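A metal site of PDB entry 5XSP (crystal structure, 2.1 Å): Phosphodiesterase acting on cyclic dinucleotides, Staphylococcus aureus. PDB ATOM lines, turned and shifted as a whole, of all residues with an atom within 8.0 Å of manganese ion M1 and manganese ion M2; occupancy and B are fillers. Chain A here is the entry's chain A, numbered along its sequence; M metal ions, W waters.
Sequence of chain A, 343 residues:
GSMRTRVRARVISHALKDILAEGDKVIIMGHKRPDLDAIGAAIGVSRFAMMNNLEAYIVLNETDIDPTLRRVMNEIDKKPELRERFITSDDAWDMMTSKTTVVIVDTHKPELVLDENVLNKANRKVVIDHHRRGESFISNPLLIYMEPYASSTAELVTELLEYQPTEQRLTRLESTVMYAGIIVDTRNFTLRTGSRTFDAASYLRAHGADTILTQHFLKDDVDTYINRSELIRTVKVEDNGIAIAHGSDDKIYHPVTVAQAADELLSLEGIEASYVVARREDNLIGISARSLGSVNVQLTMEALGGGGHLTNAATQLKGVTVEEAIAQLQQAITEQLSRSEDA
OD2 of Asp 37 is bound to manganese ion M1, 2.3 Å away. Manganese ion M1 is bound by the side-chain carboxylate (OD2) of Asp 185. OD1 of Asp 106 binds manganese ion M1 (2.4 Å). Water W1 binds manganese ion M1, 2.4 Å away. A ring nitrogen (NE2) of His 130 is bound to manganese ion M1 (2.5 Å). Manganese ion M1 has five donor atoms within binding distance.
The nearest printed residue that does not touch manganese ion M1 is Thr 153 (4.3 Å).
The backbone NH (N) of Asp 37 lies close to the side-chain carboxylate (OD1) of Asp 35 (3.4 Å). OD1 of Asp 37 is in hydrogen-bond range of N of Thr 153 (3.3 Å). OD1 of Asp 37 lies within hydrogen-bond range of N of Ala 154, 2.8 Å away. OD1 of Asp 106 lies close to OG1 of Thr 153 (2.7 Å). OD1 of Asp 35 lies within hydrogen-bond range of N of Ala 38 (3.1 Å). ND1 of His 130 sits close to O of Ser 151. The backbone carbonyl oxygen (O) of His 130 lies within hydrogen-bond range of the guanidinium group (NH2) of Arg 192 (2.8 Å). ND1 of His 130 is in hydrogen-bond range of O of Ala 150 (3.3 Å).
The nearest printed residue that does not touch manganese ion M2 is Asp 37 (4.7 Å).
Manganese ion M2 is bound by water W1 (2.4 Å), the side-chain carboxylate of Asp 106 (2.4 Å), the side-chain carboxylate of Asp 35 (2.5 Å) and a ring nitrogen (NE2) of His 31 (2.6 Å). Manganese ion M2 has four donor atoms within binding distance. Slightly farther from manganese ion M2 lies the side-chain carboxylate (OD1) of Asp 35 (2.9 Å).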
ATOM      1  N   GLY A  30     -16.750 -20.164 -25.165  1.00  0.00           N
ATOM      2  CA  GLY A  30     -17.402 -18.982 -24.658  1.00  0.00           C
ATOM      3  C   GLY A  30     -18.652 -18.660 -25.475  1.00  0.00           C
ATOM      4  O   GLY A  30     -19.328 -19.564 -25.981  1.00  0.00           O
ATOM      5  N   HIS A  31     -18.957 -17.379 -25.606  1.00  0.00           N
ATOM      6  CA  HIS A  31     -20.134 -16.931 -26.335  1.00  0.00           C
ATOM      7  C   HIS A  31     -19.865 -16.660 -27.825  1.00  0.00           C
ATOM      8  O   HIS A  31     -18.720 -16.569 -28.252  1.00  0.00           O
ATOM      9  CB  HIS A  31     -20.723 -15.675 -25.664  1.00  0.00           C
ATOM     10  CG  HIS A  31     -19.740 -14.560 -25.492  1.00  0.00           C
ATOM     11  ND1 HIS A  31     -19.316 -13.771 -26.541  1.00  0.00           N
ATOM     12  CD2 HIS A  31     -19.108 -14.087 -24.390  1.00  0.00           C
ATOM     13  CE1 HIS A  31     -18.466 -12.869 -26.093  1.00  0.00           C
ATOM     14  NE2 HIS A  31     -18.316 -13.040 -24.789  1.00  0.00           N
ATOM     15  N   LYS A  32     -20.930 -16.541 -28.616  1.00  0.00           N
ATOM     16  CA  LYS A  32     -20.783 -16.256 -30.047  1.00  0.00           C
ATOM     17  C   LYS A  32     -20.094 -14.905 -30.213  1.00  0.00           C
ATOM     18  O   LYS A  32     -20.244 -14.018 -29.372  1.00  0.00           O
ATOM     19  CB  LYS A  32     -22.150 -16.244 -30.735  1.00  0.00           C
ATOM     20  CG  LYS A  32     -22.853 -17.607 -30.775  1.00  0.00           C
ATOM     21  CD  LYS A  32     -24.353 -17.451 -31.053  1.00  0.00           C
ATOM     22  CE  LYS A  32     -24.935 -18.653 -31.792  1.00  0.00           C
ATOM     23  NZ  LYS A  32     -24.713 -19.958 -31.113  1.00  0.00           N
ATOM     24  N   ARG A  33     -19.327 -14.755 -31.294  1.00  0.00           N
ATOM     25  CA  ARG A  33     -18.575 -13.525 -31.519  1.00  0.00           C
ATOM     26  C   ARG A  33     -17.749 -13.183 -30.261  1.00  0.00           C
ATOM     27  O   ARG A  33     -17.929 -12.125 -29.660  1.00  0.00           O
ATOM     28  CB  ARG A  33     -19.535 -12.389 -31.856  1.00  0.00           C
ATOM     29  CG  ARG A  33     -19.457 -11.941 -33.316  1.00  0.00           C
ATOM     30  CD  ARG A  33     -18.573 -10.708 -33.452  1.00  0.00           C
ATOM     31  NE  ARG A  33     -18.403 -10.269 -34.835  1.00  0.00           N
ATOM     32  CZ  ARG A  33     -17.808  -9.136 -35.186  1.00  0.00           C
ATOM     33  NH1 ARG A  33     -17.343  -8.317 -34.238  1.00  0.00           N
ATOM     34  NH2 ARG A  33     -17.666  -8.800 -36.467  1.00  0.00           N
ATOM     35  N   PRO A  34     -16.845 -14.098 -29.877  1.00  0.00           N
ATOM     36  CA  PRO A  34     -16.177 -13.980 -28.577  1.00  0.00           C
ATOM     37  C   PRO A  34     -15.301 -12.735 -28.491  1.00  0.00           C
ATOM     38  O   PRO A  34     -14.598 -12.391 -29.449  1.00  0.00           O
ATOM     39  CB  PRO A  34     -15.319 -15.237 -28.529  1.00  0.00           C
ATOM     40  CG  PRO A  34     -15.094 -15.617 -29.984  1.00  0.00           C
ATOM     41  CD  PRO A  34     -16.355 -15.237 -30.675  1.00  0.00           C
ATOM     42  N   ASP A  35     -15.364 -12.030 -27.358  1.00  0.00           N
ATOM     43  CA  ASP A  35     -14.458 -10.922 -27.110  1.00  0.00           C
ATOM     44  C   ASP A  35     -13.231 -11.439 -26.340  1.00  0.00           C
ATOM     45  O   ASP A  35     -13.073 -12.651 -26.153  1.00  0.00           O
ATOM     46  CB  ASP A  35     -15.162  -9.804 -26.343  1.00  0.00           C
ATOM     47  CG  ASP A  35     -15.820 -10.301 -25.069  1.00  0.00           C
ATOM     48  OD1 ASP A  35     -15.398 -11.354 -24.533  1.00  0.00           O
ATOM     49  OD2 ASP A  35     -16.764  -9.648 -24.599  1.00  0.00           O
ATOM     50  N   LEU A  36     -12.374 -10.527 -25.908  1.00  0.00           N
ATOM     51  CA  LEU A  36     -11.110 -10.958 -25.329  1.00  0.00           C
ATOM     52  C   LEU A  36     -11.254 -11.537 -23.921  1.00  0.00           C
ATOM     53  O   LEU A  36     -10.412 -12.306 -23.477  1.00  0.00           O
ATOM     54  CB  LEU A  36     -10.060  -9.830 -25.379  1.00  0.00           C
ATOM     55  CG  LEU A  36      -9.641  -9.439 -26.804  1.00  0.00           C
ATOM     56  CD1 LEU A  36      -8.558  -8.389 -26.789  1.00  0.00           C
ATOM     57  CD2 LEU A  36      -9.205 -10.659 -27.620  1.00  0.00           C
ATOM     58  N   ASP A  37     -12.308 -11.186 -23.194  1.00  0.00           N
ATOM     59  CA  ASP A  37     -12.541 -11.842 -21.911  1.00  0.00           C
ATOM     60  C   ASP A  37     -12.899 -13.305 -22.146  1.00  0.00           C
ATOM     61  O   ASP A  37     -12.381 -14.184 -21.474  1.00  0.00           O
ATOM     62  CB  ASP A  37     -13.630 -11.141 -21.092  1.00  0.00           C
ATOM     63  CG  ASP A  37     -13.715 -11.692 -19.670  1.00  0.00           C
ATOM     64  OD1 ASP A  37     -12.654 -12.036 -19.094  1.00  0.00           O
ATOM     65  OD2 ASP A  37     -14.834 -11.761 -19.110  1.00  0.00           O
ATOM     66  N   ALA A  38     -13.787 -13.558 -23.109  1.00  0.00           N
ATOM     67  CA  ALA A  38     -14.189 -14.921 -23.413  1.00  0.00           C
ATOM     68  C   ALA A  38     -12.957 -15.728 -23.827  1.00  0.00           C
ATOM     69  O   ALA A  38     -12.738 -16.829 -23.346  1.00  0.00           O
ATOM     70  CB  ALA A  38     -15.255 -14.952 -24.521  1.00  0.00           C
ATOM     71  N   ILE A  39     -12.136 -15.153 -24.704  1.00  0.00           N
ATOM     72  CA  ILE A  39     -10.988 -15.874 -25.197  1.00  0.00           C
ATOM     73  C   ILE A  39      -9.904 -16.001 -24.087  1.00  0.00           C
ATOM     74  O   ILE A  39      -9.320 -17.051 -23.890  1.00  0.00           O
ATOM     75  CB  ILE A  39     -10.450 -15.218 -26.462  1.00  0.00           C
ATOM     76  CG1 ILE A  39     -11.487 -15.368 -27.591  1.00  0.00           C
ATOM     77  CG2 ILE A  39      -9.124 -15.827 -26.860  1.00  0.00           C
ATOM     78  CD1 ILE A  39     -11.758 -16.821 -28.019  1.00  0.00           C
ATOM     79  N   ALA A  41     -10.376 -15.952 -20.756  1.00  0.00           N
ATOM     80  CA  ALA A  41     -10.898 -16.961 -19.834  1.00  0.00           C
ATOM     81  C   ALA A  41     -10.653 -18.375 -20.360  1.00  0.00           C
ATOM     82  O   ALA A  41     -10.218 -19.251 -19.621  1.00  0.00           O
ATOM     83  CB  ALA A  41     -12.371 -16.731 -19.587  1.00  0.00           C
ATOM     84  N   VAL A 105     -17.414 -20.572 -20.592  1.00  0.00           N
ATOM     85  CA  VAL A 105     -16.882 -19.367 -19.931  1.00  0.00           C
ATOM     86  C   VAL A 105     -17.528 -18.092 -20.459  1.00  0.00           C
ATOM     87  O   VAL A 105     -17.780 -17.952 -21.673  1.00  0.00           O
ATOM     88  CB  VAL A 105     -15.358 -19.242 -20.148  1.00  0.00           C
ATOM     89  CG1 VAL A 105     -14.629 -20.431 -19.503  1.00  0.00           C
ATOM     90  CG2 VAL A 105     -15.048 -19.191 -21.640  1.00  0.00           C
ATOM     91  N   ASP A 106     -17.820 -17.183 -19.537  1.00  0.00           N
ATOM     92  CA  ASP A 106     -18.216 -15.819 -19.860  1.00  0.00           C
ATOM     93  C   ASP A 106     -19.601 -15.729 -20.497  1.00  0.00           C
ATOM     94  O   ASP A 106     -19.959 -14.713 -21.115  1.00  0.00           O
ATOM     95  CB  ASP A 106     -17.166 -15.159 -20.748  1.00  0.00           C
ATOM     96  CG  ASP A 106     -17.215 -13.665 -20.648  1.00  0.00           C
ATOM     97  OD1 ASP A 106     -17.413 -13.152 -19.530  1.00  0.00           O
ATOM     98  OD2 ASP A 106     -17.061 -13.021 -21.688  1.00  0.00           O
ATOM     99  N   THR A 107     -20.372 -16.788 -20.327  1.00  0.00           N
ATOM    100  CA  THR A 107     -21.797 -16.747 -20.607  1.00  0.00           C
ATOM    101  C   THR A 107     -22.444 -17.904 -19.853  1.00  0.00           C
ATOM    102  O   THR A 107     -21.742 -18.806 -19.393  1.00  0.00           O
ATOM    103  CB  THR A 107     -22.060 -16.877 -22.115  1.00  0.00           C
ATOM    104  OG1 THR A 107     -23.456 -16.672 -22.363  1.00  0.00           O
ATOM    105  CG2 THR A 107     -21.651 -18.232 -22.594  1.00  0.00           C
ATOM    106  N   ASP A 129     -18.804 -17.702 -14.966  1.00  0.00           N
ATOM    107  CA  ASP A 129     -19.273 -16.442 -15.533  1.00  0.00           C
ATOM    108  C   ASP A 129     -19.399 -15.391 -14.443  1.00  0.00           C
ATOM    109  O   ASP A 129     -19.446 -15.735 -13.264  1.00  0.00           O
ATOM    110  CB  ASP A 129     -20.607 -16.668 -16.247  1.00  0.00           C
ATOM    111  CG  ASP A 129     -21.087 -15.452 -17.015  1.00  0.00           C
ATOM    112  OD1 ASP A 129     -20.265 -14.634 -17.486  1.00  0.00           O
ATOM    113  OD2 ASP A 129     -22.310 -15.335 -17.151  1.00  0.00           O
ATOM    114  N   HIS A 130     -19.454 -14.121 -14.826  1.00  0.00           N
ATOM    115  CA  HIS A 130     -19.486 -13.018 -13.864  1.00  0.00           C
ATOM    116  C   HIS A 130     -20.742 -12.157 -14.022  1.00  0.00           C
ATOM    117  O   HIS A 130     -20.743 -10.972 -13.706  1.00  0.00           O
ATOM    118  CB  HIS A 130     -18.224 -12.157 -13.963  1.00  0.00           C
ATOM    119  CG  HIS A 130     -18.092 -11.416 -15.259  1.00  0.00           C
ATOM    120  ND1 HIS A 130     -18.195 -10.049 -15.349  1.00  0.00           N
ATOM    121  CD2 HIS A 130     -17.836 -11.862 -16.522  1.00  0.00           C
ATOM    122  CE1 HIS A 130     -18.024  -9.675 -16.610  1.00  0.00           C
ATOM    123  NE2 HIS A 130     -17.812 -10.751 -17.331  1.00  0.00           N
ATOM    124  N   HIS A 131     -21.807 -12.748 -14.531  1.00  0.00           N
ATOM    125  CA  HIS A 131     -23.084 -12.057 -14.540  1.00  0.00           C
ATOM    126  C   HIS A 131     -24.016 -12.834 -13.626  1.00  0.00           C
ATOM    127  O   HIS A 131     -23.696 -13.944 -13.198  1.00  0.00           O
ATOM    128  CB  HIS A 131     -23.626 -11.976 -15.970  1.00  0.00           C
ATOM    129  CG  HIS A 131     -22.561 -11.750 -17.005  1.00  0.00           C
ATOM    130  ND1 HIS A 131     -21.800 -10.612 -17.060  1.00  0.00           N
ATOM    131  CD2 HIS A 131     -22.140 -12.538 -18.028  1.00  0.00           C
ATOM    132  CE1 HIS A 131     -20.945 -10.692 -18.071  1.00  0.00           C
ATOM    133  NE2 HIS A 131     -21.131 -11.858 -18.666  1.00  0.00           N
ATOM    134  N   ALA A 150     -17.465  -9.813  -9.835  1.00  0.00           N
ATOM    135  CA  ALA A 150     -16.132  -9.902 -10.429  1.00  0.00           C
ATOM    136  C   ALA A 150     -16.058  -9.077 -11.710  1.00  0.00           C
ATOM    137  O   ALA A 150     -17.055  -8.926 -12.409  1.00  0.00           O
ATOM    138  CB  ALA A 150     -15.777 -11.358 -10.720  1.00  0.00           C
ATOM    139  N   SER A 151     -14.887  -8.544 -12.044  1.00  0.00           N
ATOM    140  CA  SER A 151     -14.761  -7.695 -13.231  1.00  0.00           C
ATOM    141  C   SER A 151     -15.037  -8.437 -14.525  1.00  0.00           C
ATOM    142  O   SER A 151     -15.521  -7.872 -15.497  1.00  0.00           O
ATOM    143  CB  SER A 151     -13.361  -7.064 -13.326  1.00  0.00           C
ATOM    144  OG  SER A 151     -12.360  -8.056 -13.472  1.00  0.00           O
ATOM    145  N   SER A 152     -14.718  -9.733 -14.543  1.00  0.00           N
ATOM    146  CA  SER A 152     -14.577 -10.457 -15.791  1.00  0.00           C
ATOM    147  C   SER A 152     -14.415 -11.921 -15.504  1.00  0.00           C
ATOM    148  O   SER A 152     -14.143 -12.310 -14.365  1.00  0.00           O
ATOM    149  CB  SER A 152     -13.326  -9.972 -16.523  1.00  0.00           C
ATOM    150  OG  SER A 152     -12.218 -10.062 -15.638  1.00  0.00           O
ATOM    151  N   THR A 153     -14.571 -12.747 -16.534  1.00  0.00           N
ATOM    152  CA  THR A 153     -14.332 -14.169 -16.352  1.00  0.00           C
ATOM    153  C   THR A 153     -12.820 -14.406 -16.225  1.00  0.00           C
ATOM    154  O   THR A 153     -12.387 -15.312 -15.516  1.00  0.00           O
ATOM    155  CB  THR A 153     -14.980 -14.991 -17.480  1.00  0.00           C
ATOM    156  OG1 THR A 153     -16.368 -14.623 -17.559  1.00  0.00           O
ATOM    157  CG2 THR A 153     -14.867 -16.511 -17.231  1.00  0.00           C
ATOM    158  N   ALA A 154     -12.020 -13.567 -16.886  1.00  0.00           N
ATOM    159  CA  ALA A 154     -10.565 -13.726 -16.808  1.00  0.00           C
ATOM    160  C   ALA A 154     -10.099 -13.605 -15.363  1.00  0.00           C
ATOM    161  O   ALA A 154      -9.253 -14.365 -14.900  1.00  0.00           O
ATOM    162  CB  ALA A 154      -9.845 -12.704 -17.697  1.00  0.00           C
ATOM    163  N   GLY A 181      -8.367  -9.188 -21.659  1.00  0.00           N
ATOM    164  CA  GLY A 181      -9.780  -9.412 -21.347  1.00  0.00           C
ATOM    165  C   GLY A 181     -10.222  -8.621 -20.137  1.00  0.00           C
ATOM    166  O   GLY A 181     -11.344  -8.079 -20.101  1.00  0.00           O
ATOM    167  N   ILE A 182      -9.383  -8.559 -19.120  1.00  0.00           N
ATOM    168  CA  ILE A 182      -9.711  -7.750 -17.954  1.00  0.00           C
ATOM    169  C   ILE A 182      -9.754  -6.264 -18.329  1.00  0.00           C
ATOM    170  O   ILE A 182     -10.676  -5.559 -17.942  1.00  0.00           O
ATOM    171  CB  ILE A 182      -8.744  -7.982 -16.791  1.00  0.00           C
ATOM    172  CG1 ILE A 182      -8.807  -9.445 -16.345  1.00  0.00           C
ATOM    173  CG2 ILE A 182      -9.064  -7.033 -15.638  1.00  0.00           C
ATOM    174  CD1 ILE A 182      -7.999  -9.755 -15.117  1.00  0.00           C
ATOM    175  N   VAL A 184     -10.490  -4.937 -21.141  1.00  0.00           N
ATOM    176  CA  VAL A 184     -11.691  -4.626 -21.922  1.00  0.00           C
ATOM    177  C   VAL A 184     -12.934  -4.564 -21.031  1.00  0.00           C
ATOM    178  O   VAL A 184     -13.656  -3.581 -21.052  1.00  0.00           O
ATOM    179  CB  VAL A 184     -11.928  -5.637 -23.064  1.00  0.00           C
ATOM    180  CG1 VAL A 184     -13.273  -5.353 -23.770  1.00  0.00           C
ATOM    181  CG2 VAL A 184     -10.801  -5.569 -24.071  1.00  0.00           C
ATOM    182  N   ASP A 185     -13.153  -5.595 -20.238  1.00  0.00           N
ATOM    183  CA  ASP A 185     -14.324  -5.637 -19.379  1.00  0.00           C
ATOM    184  C   ASP A 185     -14.356  -4.523 -18.327  1.00  0.00           C
ATOM    185  O   ASP A 185     -15.397  -4.139 -17.866  1.00  0.00           O
ATOM    186  CB  ASP A 185     -14.423  -6.992 -18.715  1.00  0.00           C
ATOM    187  CG  ASP A 185     -15.192  -7.983 -19.560  1.00  0.00           C
ATOM    188  OD1 ASP A 185     -15.423  -7.716 -20.743  1.00  0.00           O
ATOM    189  OD2 ASP A 185     -15.551  -9.033 -19.025  1.00  0.00           O
ATOM    190  N   THR A 186     -13.198  -4.008 -17.936  1.00  0.00           N
ATOM    191  CA  THR A 186     -13.141  -2.965 -16.916  1.00  0.00           C
ATOM    192  C   THR A 186     -12.960  -1.552 -17.479  1.00  0.00           C
ATOM    193  O   THR A 186     -12.967  -0.599 -16.728  1.00  0.00           O
ATOM    194  CB  THR A 186     -12.027  -3.215 -15.877  1.00  0.00           C
ATOM    195  OG1 THR A 186     -10.755  -3.150 -16.528  1.00  0.00           O
ATOM    196  CG2 THR A 186     -12.161  -4.550 -15.215  1.00  0.00           C
ATOM    197  N   ARG A 192     -16.159  -1.832 -12.376  1.00  0.00           N
ATOM    198  CA  ARG A 192     -16.211  -3.171 -11.782  1.00  0.00           C
ATOM    199  C   ARG A 192     -14.851  -3.673 -11.330  1.00  0.00           C
ATOM    200  O   ARG A 192     -14.519  -4.852 -11.458  1.00  0.00           O
ATOM    201  CB  ARG A 192     -16.835  -4.165 -12.769  1.00  0.00           C
ATOM    202  CG  ARG A 192     -18.303  -3.870 -13.090  1.00  0.00           C
ATOM    203  CD  ARG A 192     -18.887  -4.877 -14.105  1.00  0.00           C
ATOM    204  NE  ARG A 192     -19.068  -6.202 -13.515  1.00  0.00           N
ATOM    205  CZ  ARG A 192     -19.542  -7.258 -14.178  1.00  0.00           C
ATOM    206  NH1 ARG A 192     -19.894  -7.143 -15.457  1.00  0.00           N
ATOM    207  NH2 ARG A 192     -19.677  -8.432 -13.570  1.00  0.00           N
HETATM  208 MN    MN M   1     -16.824 -10.836 -19.665  1.00  0.00          MN
HETATM  209 MN    MN M   2     -17.890 -11.233 -23.009  1.00  0.00          MN
HETATM  210  O   HOH W   1     -16.869  -9.523 -21.729  1.00  0.00           O
HETATM  211  O   HOH W   2     -19.068  -8.816 -20.243  1.00  0.00           O
